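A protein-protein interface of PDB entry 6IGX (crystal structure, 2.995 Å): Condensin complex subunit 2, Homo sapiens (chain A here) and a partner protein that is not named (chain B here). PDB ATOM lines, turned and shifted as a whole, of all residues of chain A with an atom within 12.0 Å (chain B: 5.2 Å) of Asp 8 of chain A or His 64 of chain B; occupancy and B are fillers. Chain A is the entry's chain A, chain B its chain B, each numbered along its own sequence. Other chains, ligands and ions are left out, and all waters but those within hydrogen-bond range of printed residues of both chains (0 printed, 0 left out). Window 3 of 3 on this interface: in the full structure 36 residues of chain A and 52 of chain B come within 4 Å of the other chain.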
ATOM      1  N   ILE A   3      -8.537 -16.771 -27.920  1.00  0.00           N
ATOM      2  CA  ILE A   3      -8.997 -15.598 -27.183  1.00  0.00           C
ATOM      3  C   ILE A   3      -9.422 -15.929 -25.755  1.00  0.00           C
ATOM      4  O   ILE A   3     -10.264 -16.799 -25.529  1.00  0.00           O
ATOM      5  CB  ILE A   3     -10.170 -14.910 -27.902  1.00  0.00           C
ATOM      6  CG1 ILE A   3      -9.789 -14.598 -29.350  1.00  0.00           C
ATOM      7  CG2 ILE A   3     -10.570 -13.636 -27.172  1.00  0.00           C
ATOM      8  CD1 ILE A   3     -10.833 -13.802 -30.097  1.00  0.00           C
ATOM      9  N   ASP A   4      -8.831 -15.222 -24.797  1.00  0.00           N
ATOM     10  CA  ASP A   4      -9.155 -15.398 -23.387  1.00  0.00           C
ATOM     11  C   ASP A   4     -10.198 -14.375 -22.945  1.00  0.00           C
ATOM     12  O   ASP A   4      -9.881 -13.208 -22.722  1.00  0.00           O
ATOM     13  CB  ASP A   4      -7.888 -15.273 -22.535  1.00  0.00           C
ATOM     14  CG  ASP A   4      -8.154 -15.470 -21.056  1.00  0.00           C
ATOM     15  OD1 ASP A   4      -9.118 -16.187 -20.707  1.00  0.00           O
ATOM     16  OD2 ASP A   4      -7.392 -14.907 -20.241  1.00  0.00           O
ATOM     17  N   PHE A   5     -11.443 -14.824 -22.824  1.00  0.00           N
ATOM     18  CA  PHE A   5     -12.550 -13.951 -22.444  1.00  0.00           C
ATOM     19  C   PHE A   5     -12.658 -13.765 -20.934  1.00  0.00           C
ATOM     20  O   PHE A   5     -13.593 -13.129 -20.444  1.00  0.00           O
ATOM     21  CB  PHE A   5     -13.870 -14.506 -22.982  1.00  0.00           C
ATOM     22  CG  PHE A   5     -13.979 -14.475 -24.481  1.00  0.00           C
ATOM     23  CD1 PHE A   5     -14.455 -13.349 -25.131  1.00  0.00           C
ATOM     24  CD2 PHE A   5     -13.617 -15.576 -25.237  1.00  0.00           C
ATOM     25  CE1 PHE A   5     -14.562 -13.320 -26.507  1.00  0.00           C
ATOM     26  CE2 PHE A   5     -13.721 -15.554 -26.611  1.00  0.00           C
ATOM     27  CZ  PHE A   5     -14.193 -14.424 -27.249  1.00  0.00           C
ATOM     28  N   GLU A   6     -11.704 -14.320 -20.195  1.00  0.00           N
ATOM     29  CA  GLU A   6     -11.807 -14.363 -18.743  1.00  0.00           C
ATOM     30  C   GLU A   6     -11.320 -13.083 -18.067  1.00  0.00           C
ATOM     31  O   GLU A   6     -12.061 -12.459 -17.306  1.00  0.00           O
ATOM     32  CB  GLU A   6     -11.031 -15.563 -18.205  1.00  0.00           C
ATOM     33  CG  GLU A   6     -11.527 -16.892 -18.742  1.00  0.00           C
ATOM     34  CD  GLU A   6     -12.938 -17.218 -18.290  1.00  0.00           C
ATOM     35  OE1 GLU A   6     -13.516 -16.433 -17.510  1.00  0.00           O
ATOM     36  OE2 GLU A   6     -13.473 -18.263 -18.720  1.00  0.00           O
ATOM     37  N   ASP A   7     -10.080 -12.693 -18.344  1.00  0.00           N
ATOM     38  CA  ASP A   7      -9.472 -11.551 -17.662  1.00  0.00           C
ATOM     39  C   ASP A   7     -10.142 -10.237 -18.045  1.00  0.00           C
ATOM     40  O   ASP A   7     -10.230  -9.892 -19.221  1.00  0.00           O
ATOM     41  CB  ASP A   7      -7.972 -11.472 -17.961  1.00  0.00           C
ATOM     42  CG  ASP A   7      -7.673 -11.455 -19.443  1.00  0.00           C
ATOM     43  OD1 ASP A   7      -8.515 -11.957 -20.219  1.00  0.00           O
ATOM     44  OD2 ASP A   7      -6.605 -10.932 -19.832  1.00  0.00           O
ATOM     45  N   ASP A   8     -10.633  -9.516 -17.042  1.00  0.00           N
ATOM     46  CA  ASP A   8     -11.274  -8.231 -17.282  1.00  0.00           C
ATOM     47  C   ASP A   8     -10.249  -7.209 -17.768  1.00  0.00           C
ATOM     48  O   ASP A   8      -9.500  -6.636 -16.976  1.00  0.00           O
ATOM     49  CB  ASP A   8     -11.973  -7.727 -16.014  1.00  0.00           C
ATOM     50  CG  ASP A   8     -12.685  -6.399 -16.226  1.00  0.00           C
ATOM     51  OD1 ASP A   8     -13.010  -6.072 -17.389  1.00  0.00           O
ATOM     52  OD2 ASP A   8     -12.923  -5.684 -15.227  1.00  0.00           O
ATOM     53  N   ILE A   9     -10.214  -6.997 -19.079  1.00  0.00           N
ATOM     54  CA  ILE A   9      -9.326  -6.009 -19.672  1.00  0.00           C
ATOM     55  C   ILE A   9     -10.036  -4.671 -19.833  1.00  0.00           C
ATOM     56  O   ILE A   9     -11.161  -4.615 -20.329  1.00  0.00           O
ATOM     57  CB  ILE A   9      -8.804  -6.464 -21.045  1.00  0.00           C
ATOM     58  CG1 ILE A   9      -7.776  -7.582 -20.882  1.00  0.00           C
ATOM     59  CG2 ILE A   9      -8.173  -5.294 -21.779  1.00  0.00           C
ATOM     60  CD1 ILE A   9      -6.442  -7.107 -20.347  1.00  0.00           C
ATOM     61  N   ASP A  10      -9.377  -3.599 -19.403  1.00  0.00           N
ATOM     62  CA  ASP A  10      -9.909  -2.255 -19.580  1.00  0.00           C
ATOM     63  C   ASP A  10      -9.729  -1.840 -21.034  1.00  0.00           C
ATOM     64  O   ASP A  10      -8.663  -1.365 -21.425  1.00  0.00           O
ATOM     65  CB  ASP A  10      -9.220  -1.259 -18.645  1.00  0.00           C
ATOM     66  CG  ASP A  10      -9.647   0.172 -18.906  1.00  0.00           C
ATOM     67  OD1 ASP A  10     -10.696   0.586 -18.369  1.00  0.00           O
ATOM     68  OD2 ASP A  10      -8.935   0.884 -19.645  1.00  0.00           O
ATOM     69  N   PHE A  11     -10.775  -2.030 -21.831  1.00  0.00           N
ATOM     70  CA  PHE A  11     -10.685  -1.840 -23.274  1.00  0.00           C
ATOM     71  C   PHE A  11     -10.741  -0.370 -23.665  1.00  0.00           C
ATOM     72  O   PHE A  11     -10.792  -0.043 -24.852  1.00  0.00           O
ATOM     73  CB  PHE A  11     -11.803  -2.604 -23.986  1.00  0.00           C
ATOM     74  CG  PHE A  11     -11.605  -4.092 -24.005  1.00  0.00           C
ATOM     75  CD1 PHE A  11     -10.545  -4.657 -24.696  1.00  0.00           C
ATOM     76  CD2 PHE A  11     -12.484  -4.928 -23.339  1.00  0.00           C
ATOM     77  CE1 PHE A  11     -10.362  -6.028 -24.714  1.00  0.00           C
ATOM     78  CE2 PHE A  11     -12.308  -6.298 -23.355  1.00  0.00           C
ATOM     79  CZ  PHE A  11     -11.247  -6.849 -24.043  1.00  0.00           C
ATOM     80  N   ASP A  12     -10.728   0.515 -22.672  1.00  0.00           N
ATOM     81  CA  ASP A  12     -10.789   1.948 -22.937  1.00  0.00           C
ATOM     82  C   ASP A  12      -9.582   2.419 -23.734  1.00  0.00           C
ATOM     83  O   ASP A  12      -9.708   3.282 -24.595  1.00  0.00           O
ATOM     84  CB  ASP A  12     -10.883   2.742 -21.634  1.00  0.00           C
ATOM     85  CG  ASP A  12     -10.995   4.238 -21.875  1.00  0.00           C
ATOM     86  OD1 ASP A  12     -12.011   4.672 -22.462  1.00  0.00           O
ATOM     87  OD2 ASP A  12     -10.062   4.978 -21.492  1.00  0.00           O
ATOM     88  N   VAL A  13      -8.416   1.854 -23.438  1.00  0.00           N
ATOM     89  CA  VAL A  13      -7.202   2.150 -24.193  1.00  0.00           C
ATOM     90  C   VAL A  13      -7.429   2.044 -25.699  1.00  0.00           C
ATOM     91  O   VAL A  13      -6.880   2.826 -26.476  1.00  0.00           O
ATOM     92  CB  VAL A  13      -6.050   1.206 -23.798  1.00  0.00           C
ATOM     93  CG1 VAL A  13      -4.750   1.651 -24.449  1.00  0.00           C
ATOM     94  CG2 VAL A  13      -5.901   1.154 -22.284  1.00  0.00           C
ATOM     95  N   TYR A  14      -8.246   1.073 -26.100  1.00  0.00           N
ATOM     96  CA  TYR A  14      -8.499   0.809 -27.513  1.00  0.00           C
ATOM     97  C   TYR A  14      -9.608   1.672 -28.116  1.00  0.00           C
ATOM     98  O   TYR A  14      -9.502   2.112 -29.260  1.00  0.00           O
ATOM     99  CB  TYR A  14      -8.850  -0.667 -27.713  1.00  0.00           C
ATOM    100  CG  TYR A  14      -7.746  -1.636 -27.350  1.00  0.00           C
ATOM    101  CD1 TYR A  14      -6.755  -1.965 -28.263  1.00  0.00           C
ATOM    102  CD2 TYR A  14      -7.711  -2.244 -26.102  1.00  0.00           C
ATOM    103  CE1 TYR A  14      -5.750  -2.858 -27.940  1.00  0.00           C
ATOM    104  CE2 TYR A  14      -6.711  -3.140 -25.770  1.00  0.00           C
ATOM    105  CZ  TYR A  14      -5.733  -3.443 -26.693  1.00  0.00           C
ATOM    106  OH  TYR A  14      -4.732  -4.332 -26.370  1.00  0.00           O
ATOM    107  N   PHE A  15     -10.667   1.912 -27.349  1.00  0.00           N
ATOM    108  CA  PHE A  15     -11.864   2.576 -27.868  1.00  0.00           C
ATOM    109  C   PHE A  15     -11.810   4.090 -27.691  1.00  0.00           C
ATOM    110  O   PHE A  15     -12.480   4.832 -28.411  1.00  0.00           O
ATOM    111  CB  PHE A  15     -13.120   2.016 -27.194  1.00  0.00           C
ATOM    112  CG  PHE A  15     -13.553   0.679 -27.727  1.00  0.00           C
ATOM    113  CD1 PHE A  15     -14.433   0.593 -28.796  1.00  0.00           C
ATOM    114  CD2 PHE A  15     -13.077  -0.496 -27.164  1.00  0.00           C
ATOM    115  CE1 PHE A  15     -14.833  -0.638 -29.290  1.00  0.00           C
ATOM    116  CE2 PHE A  15     -13.470  -1.728 -27.654  1.00  0.00           C
ATOM    117  CZ  PHE A  15     -14.350  -1.800 -28.719  1.00  0.00           C
ATOM    118  N   GLU B  60     -25.794  -5.252 -22.601  1.00  0.00           N
ATOM    119  CA  GLU B  60     -24.526  -4.729 -22.111  1.00  0.00           C
ATOM    120  C   GLU B  60     -23.499  -5.851 -21.995  1.00  0.00           C
ATOM    121  O   GLU B  60     -22.298  -5.624 -22.143  1.00  0.00           O
ATOM    122  CB  GLU B  60     -24.718  -4.027 -20.764  1.00  0.00           C
ATOM    123  CG  GLU B  60     -25.829  -2.985 -20.768  1.00  0.00           C
ATOM    124  CD  GLU B  60     -25.891  -2.182 -19.482  1.00  0.00           C
ATOM    125  OE1 GLU B  60     -25.389  -2.673 -18.449  1.00  0.00           O
ATOM    126  OE2 GLU B  60     -26.445  -1.062 -19.505  1.00  0.00           O
ATOM    127  N   GLU B  61     -23.978  -7.062 -21.727  1.00  0.00           N
ATOM    128  CA  GLU B  61     -23.113  -8.235 -21.659  1.00  0.00           C
ATOM    129  C   GLU B  61     -22.552  -8.622 -23.025  1.00  0.00           C
ATOM    130  O   GLU B  61     -21.391  -9.010 -23.143  1.00  0.00           O
ATOM    131  CB  GLU B  61     -23.873  -9.424 -21.069  1.00  0.00           C
ATOM    132  CG  GLU B  61     -23.770  -9.556 -19.566  1.00  0.00           C
ATOM    133  CD  GLU B  61     -23.312 -10.938 -19.144  1.00  0.00           C
ATOM    134  OE1 GLU B  61     -24.125 -11.885 -19.217  1.00  0.00           O
ATOM    135  OE2 GLU B  61     -22.136 -11.081 -18.749  1.00  0.00           O
ATOM    136  N   PHE B  62     -23.388  -8.517 -24.052  1.00  0.00           N
ATOM    137  CA  PHE B  62     -23.006  -8.911 -25.403  1.00  0.00           C
ATOM    138  C   PHE B  62     -21.876  -8.048 -25.953  1.00  0.00           C
ATOM    139  O   PHE B  62     -20.896  -8.559 -26.496  1.00  0.00           O
ATOM    140  CB  PHE B  62     -24.216  -8.841 -26.336  1.00  0.00           C
ATOM    141  CG  PHE B  62     -24.035  -9.588 -27.623  1.00  0.00           C
ATOM    142  CD1 PHE B  62     -24.081 -10.971 -27.649  1.00  0.00           C
ATOM    143  CD2 PHE B  62     -23.824  -8.908 -28.810  1.00  0.00           C
ATOM    144  CE1 PHE B  62     -23.918 -11.662 -28.836  1.00  0.00           C
ATOM    145  CE2 PHE B  62     -23.661  -9.592 -29.998  1.00  0.00           C
ATOM    146  CZ  PHE B  62     -23.708 -10.972 -30.011  1.00  0.00           C
ATOM    147  N   ILE B  63     -22.026  -6.736 -25.813  1.00  0.00           N
ATOM    148  CA  ILE B  63     -21.025  -5.792 -26.291  1.00  0.00           C
ATOM    149  C   ILE B  63     -19.708  -5.924 -25.532  1.00  0.00           C
ATOM    150  O   ILE B  63     -18.635  -5.748 -26.107  1.00  0.00           O
ATOM    151  CB  ILE B  63     -21.525  -4.341 -26.174  1.00  0.00           C
ATOM    152  CG1 ILE B  63     -22.865  -4.181 -26.899  1.00  0.00           C
ATOM    153  CG2 ILE B  63     -20.488  -3.371 -26.720  1.00  0.00           C
ATOM    154  CD1 ILE B  63     -22.920  -4.857 -28.250  1.00  0.00           C
ATOM    155  N   HIS B  64     -19.794  -6.229 -24.241  1.00  0.00           N
ATOM    156  CA  HIS B  64     -18.605  -6.318 -23.398  1.00  0.00           C
ATOM    157  C   HIS B  64     -17.639  -7.407 -23.856  1.00  0.00           C
ATOM    158  O   HIS B  64     -16.425  -7.198 -23.881  1.00  0.00           O
ATOM    159  CB  HIS B  64     -18.996  -6.565 -21.940  1.00  0.00           C
ATOM    160  CG  HIS B  64     -17.831  -6.856 -21.048  1.00  0.00           C
ATOM    161  ND1 HIS B  64     -17.295  -8.119 -20.913  1.00  0.00           N
ATOM    162  CD2 HIS B  64     -17.090  -6.047 -20.255  1.00  0.00           C
ATOM    163  CE1 HIS B  64     -16.278  -8.076 -20.070  1.00  0.00           C
ATOM    164  NE2 HIS B  64     -16.132  -6.830 -19.656  1.00  0.00           N
ATOM    165  N   TYR B  65     -18.177  -8.566 -24.216  1.00  0.00           N
ATOM    166  CA  TYR B  65     -17.338  -9.685 -24.627  1.00  0.00           C
ATOM    167  C   TYR B  65     -17.013  -9.600 -26.108  1.00  0.00           C
ATOM    168  O   TYR B  65     -16.057 -10.214 -26.576  1.00  0.00           O
ATOM    169  CB  TYR B  65     -18.007 -11.019 -24.295  1.00  0.00           C
ATOM    170  CG  TYR B  65     -17.925 -11.366 -22.826  1.00  0.00           C
ATOM    171  CD1 TYR B  65     -16.771 -11.924 -22.290  1.00  0.00           C
ATOM    172  CD2 TYR B  65     -18.994 -11.130 -21.973  1.00  0.00           C
ATOM    173  CE1 TYR B  65     -16.685 -12.239 -20.949  1.00  0.00           C
ATOM    174  CE2 TYR B  65     -18.918 -11.443 -20.629  1.00  0.00           C
ATOM    175  CZ  TYR B  65     -17.761 -11.997 -20.123  1.00  0.00           C
ATOM    176  OH  TYR B  65     -17.679 -12.311 -18.785  1.00  0.00           O
ATOM    177  N   LEU B  66     -17.814  -8.838 -26.844  1.00  0.00           N
ATOM    178  CA  LEU B  66     -17.530  -8.586 -28.248  1.00  0.00           C
ATOM    179  C   LEU B  66     -16.289  -7.709 -28.377  1.00  0.00           C
ATOM    180  O   LEU B  66     -15.589  -7.748 -29.386  1.00  0.00           O
ATOM    181  CB  LEU B  66     -18.720  -7.924 -28.936  1.00  0.00           C
ATOM    182  CG  LEU B  66     -18.592  -7.820 -30.455  1.00  0.00           C
ATOM    183  CD1 LEU B  66     -18.502  -9.206 -31.072  1.00  0.00           C
ATOM    184  CD2 LEU B  66     -19.753  -7.035 -31.045  1.00  0.00           C
ATOM    185  N   LYS B  67     -16.026  -6.914 -27.344  1.00  0.00           N
ATOM    186  CA  LYS B  67     -14.866  -6.029 -27.328  1.00  0.00           C
ATOM    187  C   LYS B  67     -13.552  -6.803 -27.406  1.00  0.00           C
ATOM    188  O   LYS B  67     -12.544  -6.277 -27.881  1.00  0.00           O
ATOM    189  CB  LYS B  67     -14.873  -5.156 -26.068  1.00  0.00           C
ATOM    190  CG  LYS B  67     -15.944  -4.076 -26.049  1.00  0.00           C
ATOM    191  CD  LYS B  67     -15.781  -3.168 -24.837  1.00  0.00           C
ATOM    192  CE  LYS B  67     -16.793  -2.032 -24.845  1.00  0.00           C
ATOM    193  NZ  LYS B  67     -16.417  -0.959 -23.882  1.00  0.00           N
ATOM    194  N   TYR B  68     -13.561  -8.047 -26.936  1.00  0.00           N
ATOM    195  CA  TYR B  68     -12.343  -8.850 -26.914  1.00  0.00           C
ATOM    196  C   TYR B  68     -11.884  -9.232 -28.320  1.00  0.00           C
ATOM    197  O   TYR B  68     -10.732  -9.616 -28.517  1.00  0.00           O
ATOM    198  CB  TYR B  68     -12.550 -10.130 -26.096  1.00  0.00           C
ATOM    199  CG  TYR B  68     -12.548  -9.957 -24.592  1.00  0.00           C
ATOM    200  CD1 TYR B  68     -13.615  -9.357 -23.937  1.00  0.00           C
ATOM    201  CD2 TYR B  68     -11.485 -10.412 -23.826  1.00  0.00           C
ATOM    202  CE1 TYR B  68     -13.619  -9.211 -22.560  1.00  0.00           C
ATOM    203  CE2 TYR B  68     -11.479 -10.267 -22.450  1.00  0.00           C
ATOM    204  CZ  TYR B  68     -12.547  -9.666 -21.823  1.00  0.00           C
ATOM    205  OH  TYR B  68     -12.539  -9.524 -20.454  1.00  0.00           O
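Among the printed residues, no Asp or Glu carboxylate lies within 4 Å of a Lys or Arg side-chain nitrogen of the other chain.
The backbone NH (N) of Glu 6 of chain A sits close to the side-chain carboxylate (OD1) of Asp 4 of chain A (3.2 Å).
Of chain B, only His 64 (3.9 Å) and Tyr 68 (3.7 Å) come within 4 Å of Asp 8 of chain A. Glu 61 of chain B touches none of the printed residues of chain A. No residue of chain A comes within 4 Å of Ile 63 of chain B. Tyr 65 of chain B touches one residue of chain A. No residue of chain A comes within 4 Å of Leu 66 of chain B. Of the printed residues of chain B, Ile 9 of chain A touches Tyr 68. Of the printed residues of chain B, Phe 11 of chain A touches Lys 67 (3.6 Å) and Tyr 68 (3.3 Å). Printed residues of chain B within 4 Å of Phe 5 of chain A: Tyr 65 (3.3 Å) and Tyr 68 (3.8 Å). Of the printed residues of chain B, Phe 15 of chain A touches Lys 67. Of the printed residues of chain B, Asp 4 of chain A touches Tyr 68 (3.4 Å). Asp 12 of chain A touches none of the printed residues of chain B. The nearest printed residue of chain B that does not touch Asp 8 of chain A is Tyr 65 of chain B (7.7 Å).
O of Asp 7 of chain A sits at hydrogen-bond distance from OH of Tyr 68 of chain B, at 2.6 Å.
Tyr 68 of chain B touches Asp 4 of chain A. Tyr 65 of chain B touches Phe 5 of chain A (CE1 to O, 3.3 Å). Tyr 68 of chain B touches Phe 5 of chain A (OH to O, 3.8 Å). His 64 of chain B touches Asp 8 of chain A. Asp 8 of chain A touches Tyr 68 of chain B. Tyr 68 of chain B touches Ile 9 of chain A. CD2 of Phe 11 of chain A touches CB of Lys 67 of chain B (3.6 Å). CE2 of Phe 11 of chain A touches CE1 of Tyr 68 of chain B (3.3 Å). Phe 15 of chain A touches Lys 67 of chain B (CE2 to CG, 3.8 Å).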
